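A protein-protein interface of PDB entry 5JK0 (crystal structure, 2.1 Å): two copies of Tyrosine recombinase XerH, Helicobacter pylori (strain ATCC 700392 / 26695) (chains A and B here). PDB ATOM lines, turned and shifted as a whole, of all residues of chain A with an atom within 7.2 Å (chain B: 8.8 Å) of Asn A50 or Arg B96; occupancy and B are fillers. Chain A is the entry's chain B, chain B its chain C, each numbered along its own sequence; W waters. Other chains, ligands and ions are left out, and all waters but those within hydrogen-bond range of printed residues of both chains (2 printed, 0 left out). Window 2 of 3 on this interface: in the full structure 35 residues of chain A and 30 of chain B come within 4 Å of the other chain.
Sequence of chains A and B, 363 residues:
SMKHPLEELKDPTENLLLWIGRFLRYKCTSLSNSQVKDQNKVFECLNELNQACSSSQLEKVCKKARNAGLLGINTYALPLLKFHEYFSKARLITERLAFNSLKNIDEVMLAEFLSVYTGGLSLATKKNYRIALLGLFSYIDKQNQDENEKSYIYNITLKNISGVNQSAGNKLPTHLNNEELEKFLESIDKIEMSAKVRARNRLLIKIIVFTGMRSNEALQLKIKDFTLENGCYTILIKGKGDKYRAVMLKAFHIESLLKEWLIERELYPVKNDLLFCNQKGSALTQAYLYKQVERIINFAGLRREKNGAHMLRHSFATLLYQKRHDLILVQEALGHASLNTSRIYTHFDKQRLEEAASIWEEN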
ATOM      1  N   GLY A  21     -20.540  -8.998 -14.698  1.00  0.00           N
ATOM      2  CA  GLY A  21     -20.354 -10.325 -14.139  1.00  0.00           C
ATOM      3  C   GLY A  21     -19.007 -10.925 -14.495  1.00  0.00           C
ATOM      4  O   GLY A  21     -18.379 -11.597 -13.677  1.00  0.00           O
ATOM      5  N   ARG A  25     -15.956 -11.697 -11.787  1.00  0.00           N
ATOM      6  CA  ARG A  25     -15.392 -13.040 -11.725  1.00  0.00           C
ATOM      7  C   ARG A  25     -13.873 -12.971 -11.816  1.00  0.00           C
ATOM      8  O   ARG A  25     -13.160 -13.685 -11.106  1.00  0.00           O
ATOM      9  CB  ARG A  25     -15.939 -13.925 -12.846  1.00  0.00           C
ATOM     10  CG  ARG A  25     -15.413 -15.352 -12.794  1.00  0.00           C
ATOM     11  CD  ARG A  25     -15.378 -15.997 -14.168  1.00  0.00           C
ATOM     12  NE  ARG A  25     -14.524 -15.260 -15.095  1.00  0.00           N
ATOM     13  CZ  ARG A  25     -13.204 -15.401 -15.175  1.00  0.00           C
ATOM     14  NH1 ARG A  25     -12.574 -16.254 -14.377  1.00  0.00           N
ATOM     15  NH2 ARG A  25     -12.511 -14.686 -16.052  1.00  0.00           N
ATOM     16  N   THR A  29     -10.652 -13.755  -8.943  1.00  0.00           N
ATOM     17  CA  THR A  29      -9.567 -14.660  -9.292  1.00  0.00           C
ATOM     18  C   THR A  29      -8.206 -13.989  -9.097  1.00  0.00           C
ATOM     19  O   THR A  29      -7.207 -14.657  -8.834  1.00  0.00           O
ATOM     20  CB  THR A  29      -9.702 -15.147 -10.753  1.00  0.00           C
ATOM     21  OG1 THR A  29     -11.035 -15.627 -10.979  1.00  0.00           O
ATOM     22  CG2 THR A  29      -8.711 -16.262 -11.050  1.00  0.00           C
ATOM     23  N   GLU A  44     -17.901 -22.069  -4.668  1.00  0.00           N
ATOM     24  CA  GLU A  44     -19.287 -21.838  -5.062  1.00  0.00           C
ATOM     25  C   GLU A  44     -19.457 -20.492  -5.763  1.00  0.00           C
ATOM     26  O   GLU A  44     -20.243 -20.371  -6.702  1.00  0.00           O
ATOM     27  CB  GLU A  44     -20.211 -21.911  -3.843  1.00  0.00           C
ATOM     28  CG  GLU A  44     -20.278 -23.285  -3.195  1.00  0.00           C
ATOM     29  CD  GLU A  44     -21.144 -23.298  -1.951  1.00  0.00           C
ATOM     30  OE1 GLU A  44     -21.409 -24.395  -1.418  1.00  0.00           O
ATOM     31  OE2 GLU A  44     -21.559 -22.207  -1.505  1.00  0.00           O
ATOM     32  N   CYS A  45     -18.714 -19.489  -5.306  1.00  0.00           N
ATOM     33  CA  CYS A  45     -18.797 -18.149  -5.878  1.00  0.00           C
ATOM     34  C   CYS A  45     -18.327 -18.118  -7.330  1.00  0.00           C
ATOM     35  O   CYS A  45     -18.965 -17.501  -8.184  1.00  0.00           O
ATOM     36  CB  CYS A  45     -17.978 -17.154  -5.049  1.00  0.00           C
ATOM     37  SG  CYS A  45     -18.697 -16.732  -3.443  1.00  0.00           S
ATOM     38  N   LEU A  46     -17.209 -18.781  -7.609  1.00  0.00           N
ATOM     39  CA  LEU A  46     -16.653 -18.788  -8.957  1.00  0.00           C
ATOM     40  C   LEU A  46     -17.540 -19.563  -9.928  1.00  0.00           C
ATOM     41  O   LEU A  46     -17.618 -19.224 -11.109  1.00  0.00           O
ATOM     42  CB  LEU A  46     -15.237 -19.368  -8.952  1.00  0.00           C
ATOM     43  CG  LEU A  46     -14.145 -18.470  -8.364  1.00  0.00           C
ATOM     44  CD1 LEU A  46     -12.780 -19.125  -8.500  1.00  0.00           C
ATOM     45  CD2 LEU A  46     -14.153 -17.103  -9.029  1.00  0.00           C
ATOM     46  N   ASN A  47     -18.211 -20.598  -9.430  1.00  0.00           N
ATOM     47  CA  ASN A  47     -19.140 -21.365 -10.253  1.00  0.00           C
ATOM     48  C   ASN A  47     -20.338 -20.525 -10.682  1.00  0.00           C
ATOM     49  O   ASN A  47     -20.757 -20.568 -11.841  1.00  0.00           O
ATOM     50  CB  ASN A  47     -19.622 -22.612  -9.508  1.00  0.00           C
ATOM     51  CG  ASN A  47     -18.560 -23.693  -9.430  1.00  0.00           C
ATOM     52  OD1 ASN A  47     -17.649 -23.745 -10.257  1.00  0.00           O
ATOM     53  ND2 ASN A  47     -18.674 -24.564  -8.434  1.00  0.00           N
ATOM     54  N   GLU A  48     -20.881 -19.759  -9.742  1.00  0.00           N
ATOM     55  CA  GLU A  48     -22.035 -18.912 -10.019  1.00  0.00           C
ATOM     56  C   GLU A  48     -21.666 -17.749 -10.937  1.00  0.00           C
ATOM     57  O   GLU A  48     -22.459 -17.342 -11.789  1.00  0.00           O
ATOM     58  CB  GLU A  48     -22.636 -18.387  -8.713  1.00  0.00           C
ATOM     59  CG  GLU A  48     -23.178 -19.482  -7.806  1.00  0.00           C
ATOM     60  CD  GLU A  48     -23.598 -18.962  -6.444  1.00  0.00           C
ATOM     61  OE1 GLU A  48     -24.816 -18.813  -6.213  1.00  0.00           O
ATOM     62  OE2 GLU A  48     -22.711 -18.707  -5.602  1.00  0.00           O
ATOM     63  N   LEU A  49     -20.454 -17.226 -10.769  1.00  0.00           N
ATOM     64  CA  LEU A  49     -19.985 -16.107 -11.579  1.00  0.00           C
ATOM     65  C   LEU A  49     -19.546 -16.548 -12.972  1.00  0.00           C
ATOM     66  O   LEU A  49     -19.195 -15.716 -13.809  1.00  0.00           O
ATOM     67  CB  LEU A  49     -18.831 -15.385 -10.879  1.00  0.00           C
ATOM     68  CG  LEU A  49     -19.193 -14.548  -9.651  1.00  0.00           C
ATOM     69  CD1 LEU A  49     -17.940 -13.986  -8.994  1.00  0.00           C
ATOM     70  CD2 LEU A  49     -20.142 -13.429 -10.041  1.00  0.00           C
ATOM     71  N   ASN A  50     -19.564 -17.853 -13.220  1.00  0.00           N
ATOM     72  CA  ASN A  50     -19.183 -18.382 -14.525  1.00  0.00           C
ATOM     73  C   ASN A  50     -20.363 -18.463 -15.490  1.00  0.00           C
ATOM     74  O   ASN A  50     -20.278 -19.110 -16.533  1.00  0.00           O
ATOM     75  CB  ASN A  50     -18.541 -19.762 -14.380  1.00  0.00           C
ATOM     76  CG  ASN A  50     -17.044 -19.732 -14.612  1.00  0.00           C
ATOM     77  OD1 ASN A  50     -16.583 -19.687 -15.753  1.00  0.00           O
ATOM     78  ND2 ASN A  50     -16.274 -19.757 -13.529  1.00  0.00           N
ATOM     79  N   GLN A  51     -21.462 -17.808 -15.131  1.00  0.00           N
ATOM     80  CA  GLN A  51     -22.630 -17.739 -16.000  1.00  0.00           C
ATOM     81  C   GLN A  51     -23.345 -16.404 -15.826  1.00  0.00           C
ATOM     82  O   GLN A  51     -22.973 -15.600 -14.972  1.00  0.00           O
ATOM     83  CB  GLN A  51     -23.588 -18.898 -15.717  1.00  0.00           C
ATOM     84  CG  GLN A  51     -24.278 -18.832 -14.365  1.00  0.00           C
ATOM     85  CD  GLN A  51     -25.262 -19.970 -14.161  1.00  0.00           C
ATOM     86  OE1 GLN A  51     -26.204 -19.859 -13.376  1.00  0.00           O
ATOM     87  NE2 GLN A  51     -25.046 -21.071 -14.870  1.00  0.00           N
ATOM     88  N   ALA A  52     -24.367 -16.171 -16.643  1.00  0.00           N
ATOM     89  CA  ALA A  52     -25.120 -14.924 -16.586  1.00  0.00           C
ATOM     90  C   ALA A  52     -25.847 -14.791 -15.254  1.00  0.00           C
ATOM     91  O   ALA A  52     -26.525 -15.718 -14.812  1.00  0.00           O
ATOM     92  CB  ALA A  52     -26.107 -14.845 -17.743  1.00  0.00           C
ATOM     93  N   CYS A  53     -25.692 -13.636 -14.615  1.00  0.00           N
ATOM     94  CA  CYS A  53     -26.326 -13.380 -13.328  1.00  0.00           C
ATOM     95  C   CYS A  53     -27.167 -12.110 -13.357  1.00  0.00           C
ATOM     96  O   CYS A  53     -26.877 -11.178 -14.108  1.00  0.00           O
ATOM     97  CB  CYS A  53     -25.272 -13.270 -12.224  1.00  0.00           C
ATOM     98  SG  CYS A  53     -24.342 -14.782 -11.890  1.00  0.00           S
ATOM     99  N   PRO B  12     -12.851 -37.635 -19.263  1.00  0.00           N
ATOM    100  CA  PRO B  12     -11.686 -36.747 -19.182  1.00  0.00           C
ATOM    101  C   PRO B  12     -11.140 -36.637 -17.760  1.00  0.00           C
ATOM    102  O   PRO B  12      -9.939 -36.427 -17.577  1.00  0.00           O
ATOM    103  CB  PRO B  12     -12.234 -35.399 -19.664  1.00  0.00           C
ATOM    104  CG  PRO B  12     -13.708 -35.488 -19.451  1.00  0.00           C
ATOM    105  CD  PRO B  12     -14.055 -36.920 -19.714  1.00  0.00           C
ATOM    106  N   TYR B  86     -10.645 -30.873  -7.817  1.00  0.00           N
ATOM    107  CA  TYR B  86     -11.308 -29.691  -8.361  1.00  0.00           C
ATOM    108  C   TYR B  86     -11.989 -29.999  -9.690  1.00  0.00           C
ATOM    109  O   TYR B  86     -13.179 -29.741  -9.861  1.00  0.00           O
ATOM    110  CB  TYR B  86     -10.305 -28.547  -8.539  1.00  0.00           C
ATOM    111  CG  TYR B  86     -10.802 -27.421  -9.422  1.00  0.00           C
ATOM    112  CD1 TYR B  86     -11.676 -26.458  -8.930  1.00  0.00           C
ATOM    113  CD2 TYR B  86     -10.392 -27.318 -10.747  1.00  0.00           C
ATOM    114  CE1 TYR B  86     -12.131 -25.428  -9.733  1.00  0.00           C
ATOM    115  CE2 TYR B  86     -10.844 -26.294 -11.560  1.00  0.00           C
ATOM    116  CZ  TYR B  86     -11.711 -25.351 -11.048  1.00  0.00           C
ATOM    117  OH  TYR B  86     -12.160 -24.329 -11.851  1.00  0.00           O
ATOM    118  N   PHE B  87     -11.221 -30.555 -10.623  1.00  0.00           N
ATOM    119  CA  PHE B  87     -11.716 -30.874 -11.958  1.00  0.00           C
ATOM    120  C   PHE B  87     -12.904 -31.830 -11.907  1.00  0.00           C
ATOM    121  O   PHE B  87     -13.888 -31.650 -12.625  1.00  0.00           O
ATOM    122  CB  PHE B  87     -10.591 -31.478 -12.805  1.00  0.00           C
ATOM    123  CG  PHE B  87     -10.928 -31.615 -14.266  1.00  0.00           C
ATOM    124  CD1 PHE B  87     -11.586 -32.740 -14.739  1.00  0.00           C
ATOM    125  CD2 PHE B  87     -10.573 -30.625 -15.167  1.00  0.00           C
ATOM    126  CE1 PHE B  87     -11.894 -32.868 -16.080  1.00  0.00           C
ATOM    127  CE2 PHE B  87     -10.877 -30.749 -16.511  1.00  0.00           C
ATOM    128  CZ  PHE B  87     -11.539 -31.872 -16.967  1.00  0.00           C
ATOM    129  N   LYS B  89     -15.209 -32.611  -9.420  1.00  0.00           N
ATOM    130  CA  LYS B  89     -16.478 -32.149  -8.870  1.00  0.00           C
ATOM    131  C   LYS B  89     -17.036 -30.957  -9.648  1.00  0.00           C
ATOM    132  O   LYS B  89     -18.250 -30.780  -9.722  1.00  0.00           O
ATOM    133  CB  LYS B  89     -16.332 -31.798  -7.385  1.00  0.00           C
ATOM    134  CG  LYS B  89     -15.426 -30.621  -7.078  1.00  0.00           C
ATOM    135  CD  LYS B  89     -15.393 -30.341  -5.579  1.00  0.00           C
ATOM    136  CE  LYS B  89     -14.556 -29.110  -5.256  1.00  0.00           C
ATOM    137  NZ  LYS B  89     -14.497 -28.841  -3.789  1.00  0.00           N
ATOM    138  N   ALA B  90     -16.156 -30.151 -10.234  1.00  0.00           N
ATOM    139  CA  ALA B  90     -16.602 -29.017 -11.041  1.00  0.00           C
ATOM    140  C   ALA B  90     -17.300 -29.504 -12.308  1.00  0.00           C
ATOM    141  O   ALA B  90     -18.257 -28.888 -12.782  1.00  0.00           O
ATOM    142  CB  ALA B  90     -15.433 -28.116 -11.393  1.00  0.00           C
ATOM    143  N   ARG B  91     -16.817 -30.620 -12.845  1.00  0.00           N
ATOM    144  CA  ARG B  91     -17.400 -31.213 -14.042  1.00  0.00           C
ATOM    145  C   ARG B  91     -18.781 -31.801 -13.766  1.00  0.00           C
ATOM    146  O   ARG B  91     -19.725 -31.575 -14.524  1.00  0.00           O
ATOM    147  CB  ARG B  91     -16.472 -32.295 -14.601  1.00  0.00           C
ATOM    148  CG  ARG B  91     -17.049 -33.067 -15.777  1.00  0.00           C
ATOM    149  CD  ARG B  91     -16.041 -34.061 -16.330  1.00  0.00           C
ATOM    150  NE  ARG B  91     -16.615 -34.886 -17.388  1.00  0.00           N
ATOM    151  CZ  ARG B  91     -17.199 -36.062 -17.183  1.00  0.00           C
ATOM    152  NH1 ARG B  91     -17.696 -36.747 -18.204  1.00  0.00           N
ATOM    153  NH2 ARG B  91     -17.285 -36.557 -15.956  1.00  0.00           N
ATOM    154  N   LEU B  92     -18.895 -32.552 -12.675  1.00  0.00           N
ATOM    155  CA  LEU B  92     -20.146 -33.222 -12.336  1.00  0.00           C
ATOM    156  C   LEU B  92     -21.227 -32.239 -11.888  1.00  0.00           C
ATOM    157  O   LEU B  92     -22.416 -32.476 -12.102  1.00  0.00           O
ATOM    158  CB  LEU B  92     -19.910 -34.267 -11.243  1.00  0.00           C
ATOM    159  CG  LEU B  92     -19.053 -35.478 -11.622  1.00  0.00           C
ATOM    160  CD1 LEU B  92     -18.846 -36.387 -10.419  1.00  0.00           C
ATOM    161  CD2 LEU B  92     -19.682 -36.247 -12.773  1.00  0.00           C
ATOM    162  N   ILE B  93     -20.812 -31.137 -11.271  1.00  0.00           N
ATOM    163  CA  ILE B  93     -21.757 -30.170 -10.720  1.00  0.00           C
ATOM    164  C   ILE B  93     -22.196 -29.122 -11.742  1.00  0.00           C
ATOM    165  O   ILE B  93     -23.392 -28.916 -11.951  1.00  0.00           O
ATOM    166  CB  ILE B  93     -21.161 -29.450  -9.490  1.00  0.00           C
ATOM    167  CG1 ILE B  93     -21.028 -30.426  -8.319  1.00  0.00           C
ATOM    168  CG2 ILE B  93     -22.026 -28.265  -9.088  1.00  0.00           C
ATOM    169  CD1 ILE B  93     -20.302 -29.851  -7.122  1.00  0.00           C
ATOM    170  N   THR B  94     -21.231 -28.468 -12.378  1.00  0.00           N
ATOM    171  CA  THR B  94     -21.526 -27.341 -13.261  1.00  0.00           C
ATOM    172  C   THR B  94     -21.831 -27.773 -14.692  1.00  0.00           C
ATOM    173  O   THR B  94     -22.587 -27.105 -15.397  1.00  0.00           O
ATOM    174  CB  THR B  94     -20.358 -26.341 -13.296  1.00  0.00           C
ATOM    175  OG1 THR B  94     -19.272 -26.899 -14.044  1.00  0.00           O
ATOM    176  CG2 THR B  94     -19.889 -26.019 -11.883  1.00  0.00           C
ATOM    177  N   GLU B  95     -21.224 -28.880 -15.112  1.00  0.00           N
ATOM    178  CA  GLU B  95     -21.370 -29.399 -16.471  1.00  0.00           C
ATOM    179  C   GLU B  95     -20.969 -28.372 -17.528  1.00  0.00           C
ATOM    180  O   GLU B  95     -21.488 -28.392 -18.645  1.00  0.00           O
ATOM    181  CB  GLU B  95     -22.808 -29.867 -16.722  1.00  0.00           C
ATOM    182  CG  GLU B  95     -23.257 -31.011 -15.833  1.00  0.00           C
ATOM    183  CD  GLU B  95     -24.695 -31.416 -16.090  1.00  0.00           C
ATOM    184  OE1 GLU B  95     -25.155 -32.401 -15.476  1.00  0.00           O
ATOM    185  OE2 GLU B  95     -25.366 -30.747 -16.905  1.00  0.00           O
ATOM    186  N   ARG B  96     -20.049 -27.480 -17.176  1.00  0.00           N
ATOM    187  CA  ARG B  96     -19.554 -26.492 -18.127  1.00  0.00           C
ATOM    188  C   ARG B  96     -18.744 -27.180 -19.220  1.00  0.00           C
ATOM    189  O   ARG B  96     -18.101 -28.203 -18.977  1.00  0.00           O
ATOM    190  CB  ARG B  96     -18.712 -25.423 -17.421  1.00  0.00           C
ATOM    191  CG  ARG B  96     -19.516 -24.539 -16.478  1.00  0.00           C
ATOM    192  CD  ARG B  96     -18.839 -23.198 -16.221  1.00  0.00           C
ATOM    193  NE  ARG B  96     -17.664 -23.306 -15.361  1.00  0.00           N
ATOM    194  CZ  ARG B  96     -16.424 -23.025 -15.748  1.00  0.00           C
ATOM    195  NH1 ARG B  96     -15.417 -23.149 -14.893  1.00  0.00           N
ATOM    196  NH2 ARG B  96     -16.189 -22.615 -16.987  1.00  0.00           N
ATOM    197  N   LEU B  97     -18.781 -26.611 -20.421  1.00  0.00           N
ATOM    198  CA  LEU B  97     -18.130 -27.206 -21.585  1.00  0.00           C
ATOM    199  C   LEU B  97     -16.615 -27.305 -21.427  1.00  0.00           C
ATOM    200  O   LEU B  97     -15.962 -28.081 -22.125  1.00  0.00           O
ATOM    201  CB  LEU B  97     -18.465 -26.401 -22.843  1.00  0.00           C
ATOM    202  N   ALA B  98     -16.061 -26.524 -20.506  1.00  0.00           N
ATOM    203  CA  ALA B  98     -14.618 -26.483 -20.301  1.00  0.00           C
ATOM    204  C   ALA B  98     -14.079 -27.762 -19.661  1.00  0.00           C
ATOM    205  O   ALA B  98     -12.866 -27.958 -19.585  1.00  0.00           O
ATOM    206  CB  ALA B  98     -14.245 -25.276 -19.453  1.00  0.00           C
ATOM    207  N   PHE B  99     -14.975 -28.631 -19.203  1.00  0.00           N
ATOM    208  CA  PHE B  99     -14.563 -29.869 -18.548  1.00  0.00           C
ATOM    209  C   PHE B  99     -14.891 -31.102 -19.389  1.00  0.00           C
ATOM    210  O   PHE B  99     -14.809 -32.230 -18.903  1.00  0.00           O
ATOM    211  CB  PHE B  99     -15.223 -29.987 -17.172  1.00  0.00           C
ATOM    212  CG  PHE B  99     -14.899 -28.850 -16.245  1.00  0.00           C
ATOM    213  CD1 PHE B  99     -13.687 -28.808 -15.575  1.00  0.00           C
ATOM    214  CD2 PHE B  99     -15.806 -27.824 -16.043  1.00  0.00           C
ATOM    215  CE1 PHE B  99     -13.385 -27.761 -14.722  1.00  0.00           C
ATOM    216  CE2 PHE B  99     -15.510 -26.773 -15.191  1.00  0.00           C
ATOM    217  CZ  PHE B  99     -14.299 -26.742 -14.531  1.00  0.00           C
ATOM    218  N   ASN B 100     -15.256 -30.886 -20.649  1.00  0.00           N
ATOM    219  CA  ASN B 100     -15.613 -31.988 -21.536  1.00  0.00           C
ATOM    220  C   ASN B 100     -14.415 -32.558 -22.290  1.00  0.00           C
ATOM    221  O   ASN B 100     -14.541 -33.551 -23.006  1.00  0.00           O
ATOM    222  CB  ASN B 100     -16.683 -31.540 -22.533  1.00  0.00           C
ATOM    223  CG  ASN B 100     -18.040 -31.344 -21.883  1.00  0.00           C
ATOM    224  OD1 ASN B 100     -18.353 -31.970 -20.869  1.00  0.00           O
ATOM    225  ND2 ASN B 100     -18.855 -30.474 -22.466  1.00  0.00           N
ATOM    226  N   SER B 101     -13.255 -31.929 -22.127  1.00  0.00           N
ATOM    227  CA  SER B 101     -12.041 -32.387 -22.794  1.00  0.00           C
ATOM    228  C   SER B 101     -10.788 -31.877 -22.094  1.00  0.00           C
ATOM    229  O   SER B 101     -10.779 -30.774 -21.545  1.00  0.00           O
ATOM    230  CB  SER B 101     -12.033 -31.941 -24.258  1.00  0.00           C
ATOM    231  OG  SER B 101     -10.836 -32.341 -24.906  1.00  0.00           O
ATOM    232  N   ASN B 104      -9.316 -28.471 -23.059  1.00  0.00           N
ATOM    233  CA  ASN B 104      -9.953 -27.239 -22.604  1.00  0.00           C
ATOM    234  C   ASN B 104      -9.356 -26.697 -21.307  1.00  0.00           C
ATOM    235  O   ASN B 104      -9.806 -25.676 -20.788  1.00  0.00           O
ATOM    236  CB  ASN B 104     -11.456 -27.456 -22.426  1.00  0.00           C
ATOM    237  CG  ASN B 104     -12.162 -27.730 -23.736  1.00  0.00           C
ATOM    238  OD1 ASN B 104     -11.631 -27.449 -24.810  1.00  0.00           O
ATOM    239  ND2 ASN B 104     -13.371 -28.273 -23.655  1.00  0.00           N
ATOM    240  N   ASP B 106      -6.831 -24.615 -19.452  1.00  0.00           N
ATOM    241  CA  ASP B 106      -5.940 -23.499 -19.761  1.00  0.00           C
ATOM    242  C   ASP B 106      -5.565 -22.703 -18.514  1.00  0.00           C
ATOM    243  O   ASP B 106      -5.875 -23.104 -17.393  1.00  0.00           O
ATOM    244  CB  ASP B 106      -6.574 -22.573 -20.804  1.00  0.00           C
ATOM    245  CG  ASP B 106      -7.978 -22.125 -20.426  1.00  0.00           C
ATOM    246  OD1 ASP B 106      -8.372 -22.276 -19.250  1.00  0.00           O
ATOM    247  OD2 ASP B 106      -8.691 -21.613 -21.314  1.00  0.00           O
ATOM    248  N   VAL B 108      -6.686 -19.884 -17.441  1.00  0.00           N
ATOM    249  CA  VAL B 108      -7.856 -19.349 -16.753  1.00  0.00           C
ATOM    250  C   VAL B 108      -8.407 -20.359 -15.749  1.00  0.00           C
ATOM    251  O   VAL B 108      -8.673 -20.017 -14.595  1.00  0.00           O
ATOM    252  CB  VAL B 108      -8.962 -18.954 -17.750  1.00  0.00           C
ATOM    253  CG1 VAL B 108     -10.266 -18.658 -17.021  1.00  0.00           C
ATOM    254  CG2 VAL B 108      -8.523 -17.755 -18.576  1.00  0.00           C
ATOM    255  N   MET B 109      -8.568 -21.602 -16.191  1.00  0.00           N
ATOM    256  CA  MET B 109      -9.056 -22.666 -15.318  1.00  0.00           C
ATOM    257  C   MET B 109      -8.105 -22.897 -14.148  1.00  0.00           C
ATOM    258  O   MET B 109      -8.539 -23.063 -13.007  1.00  0.00           O
ATOM    259  CB  MET B 109      -9.246 -23.966 -16.103  1.00  0.00           C
ATOM    260  CG  MET B 109      -9.677 -25.145 -15.242  1.00  0.00           C
ATOM    261  SD  MET B 109      -9.757 -26.708 -16.140  1.00  0.00           S
ATOM    262  CE  MET B 109     -11.102 -26.385 -17.277  1.00  0.00           C
ATOM    263  N   LEU B 110      -6.808 -22.903 -14.439  1.00  0.00           N
ATOM    264  CA  LEU B 110      -5.794 -23.126 -13.415  1.00  0.00           C
ATOM    265  C   LEU B 110      -5.769 -21.983 -12.406  1.00  0.00           C
ATOM    266  O   LEU B 110      -5.558 -22.202 -11.213  1.00  0.00           O
ATOM    267  CB  LEU B 110      -4.413 -23.294 -14.053  1.00  0.00           C
ATOM    268  CG  LEU B 110      -4.224 -24.525 -14.942  1.00  0.00           C
ATOM    269  CD1 LEU B 110      -2.786 -24.633 -15.414  1.00  0.00           C
ATOM    270  CD2 LEU B 110      -4.642 -25.785 -14.206  1.00  0.00           C
ATOM    271  N   GLU B 112      -8.320 -20.152 -11.525  1.00  0.00           N
ATOM    272  CA  GLU B 112      -9.496 -20.285 -10.675  1.00  0.00           C
ATOM    273  C   GLU B 112      -9.297 -21.386  -9.637  1.00  0.00           C
ATOM    274  O   GLU B 112      -9.766 -21.271  -8.504  1.00  0.00           O
ATOM    275  CB  GLU B 112     -10.747 -20.564 -11.515  1.00  0.00           C
ATOM    276  CG  GLU B 112     -11.195 -19.380 -12.360  1.00  0.00           C
ATOM    277  CD  GLU B 112     -12.544 -19.602 -13.017  1.00  0.00           C
ATOM    278  OE1 GLU B 112     -13.173 -20.649 -12.758  1.00  0.00           O
ATOM    279  OE2 GLU B 112     -12.977 -18.723 -13.791  1.00  0.00           O
ATOM    280  N   PHE B 113      -8.598 -22.450 -10.022  1.00  0.00           N
ATOM    281  CA  PHE B 113      -8.285 -23.529  -9.092  1.00  0.00           C
ATOM    282  C   PHE B 113      -7.400 -23.031  -7.952  1.00  0.00           C
ATOM    283  O   PHE B 113      -7.632 -23.353  -6.787  1.00  0.00           O
ATOM    284  CB  PHE B 113      -7.598 -24.690  -9.814  1.00  0.00           C
ATOM    285  CG  PHE B 113      -6.782 -25.566  -8.904  1.00  0.00           C
ATOM    286  CD1 PHE B 113      -7.401 -26.426  -8.012  1.00  0.00           C
ATOM    287  CD2 PHE B 113      -5.398 -25.526  -8.939  1.00  0.00           C
ATOM    288  CE1 PHE B 113      -6.653 -27.229  -7.169  1.00  0.00           C
ATOM    289  CE2 PHE B 113      -4.645 -26.328  -8.101  1.00  0.00           C
ATOM    290  CZ  PHE B 113      -5.274 -27.180  -7.215  1.00  0.00           C
HETATM  291  O   HOH W   1     -16.560 -23.290 -12.650  1.00  0.00           O
HETATM  292  O   HOH W   2     -13.635 -19.150 -16.214  1.00  0.00           O
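The guanidinium group of Arg A25 lies within salt-bridge range of the side-chain carboxylate of Glu B112 (2.6 Å).
The side-chain amide oxygen of Asn A50 is in hydrogen-bond range of the guanidinium group of Arg B96, 3.2 Å away.
ND2 of Asn A50 lies within hydrogen-bond range of OE1 of Glu B112 (3.3 Å).
The backbone carbonyl oxygen of Arg A25 lies within hydrogen-bond range of the side-chain hydroxyl of Thr A29 (2.9 Å).
The backbone carbonyl oxygen (O) of Leu A46 lies within hydrogen-bond range of the side-chain amide nitrogen (ND2) of Asn A50, 2.8 Å away.
The side-chain hydroxyl of Thr B94 is in hydrogen-bond range of the backbone carbonyl oxygen of Ala B90 (2.6 Å).
N of Arg B96 lies close to OG1 of Thr B94 (3.3 Å).
The side-chain carboxylate (OE1) of Glu B112 lies within salt-bridge range of the guanidinium group (NH1) of Arg B96 (3.98 Å).
Glu B112 touches Thr A29.
CD1 of Leu A46 touches O of Glu B112, at 3.7 Å.
OD1 of Asn A47 touches CG2 of Thr B94 (3.6 Å).
Printed residues of chain B within 4 Å of Arg A25: Glu B112.
Of the printed residues of chain B, Thr A29 touches Glu B112 (3.9 Å).
Printed residues of chain B within 4 Å of Leu A46: Glu B112 (3.7 Å).
Asn A50 touches just these residues of chain B: Arg B96 (3.2 Å) and Glu B112 (3.3 Å).
Arg B96 touches just one residue of chain A: Asn A50 (3.2 Å).
The nearest residue of chain B that does not touch Asn A50 is Tyr B86 (6.4 Å).
The nearest printed residue of chain A that does not touch Thr B94 is Gln A51 (6.5 Å).
Of the 13 printed residues of chain A, 5 touch a printed residue of chain B.
Hydrophobic or aromatic side chains of chain A that line the printed part of chain B: Leu A46.
Along chain A the printed residues that touch a printed residue of chain B span positions 25 to 50.
Among the printed residues, 6 pairs touch across the chains.
No position is printed for both chains.
Of the 6 pairs that touch across the chains among the printed residues, none has its exchanged pair printed and touching as well.
Water W1 lies within hydrogen-bond range of NH1 of Arg B96 (2.5 Å) and OD1 of Asn A47 (2.7 Å).
Water W2 lies within hydrogen-bond range of OE2 of Glu B112 and OD1 of Asn A50.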
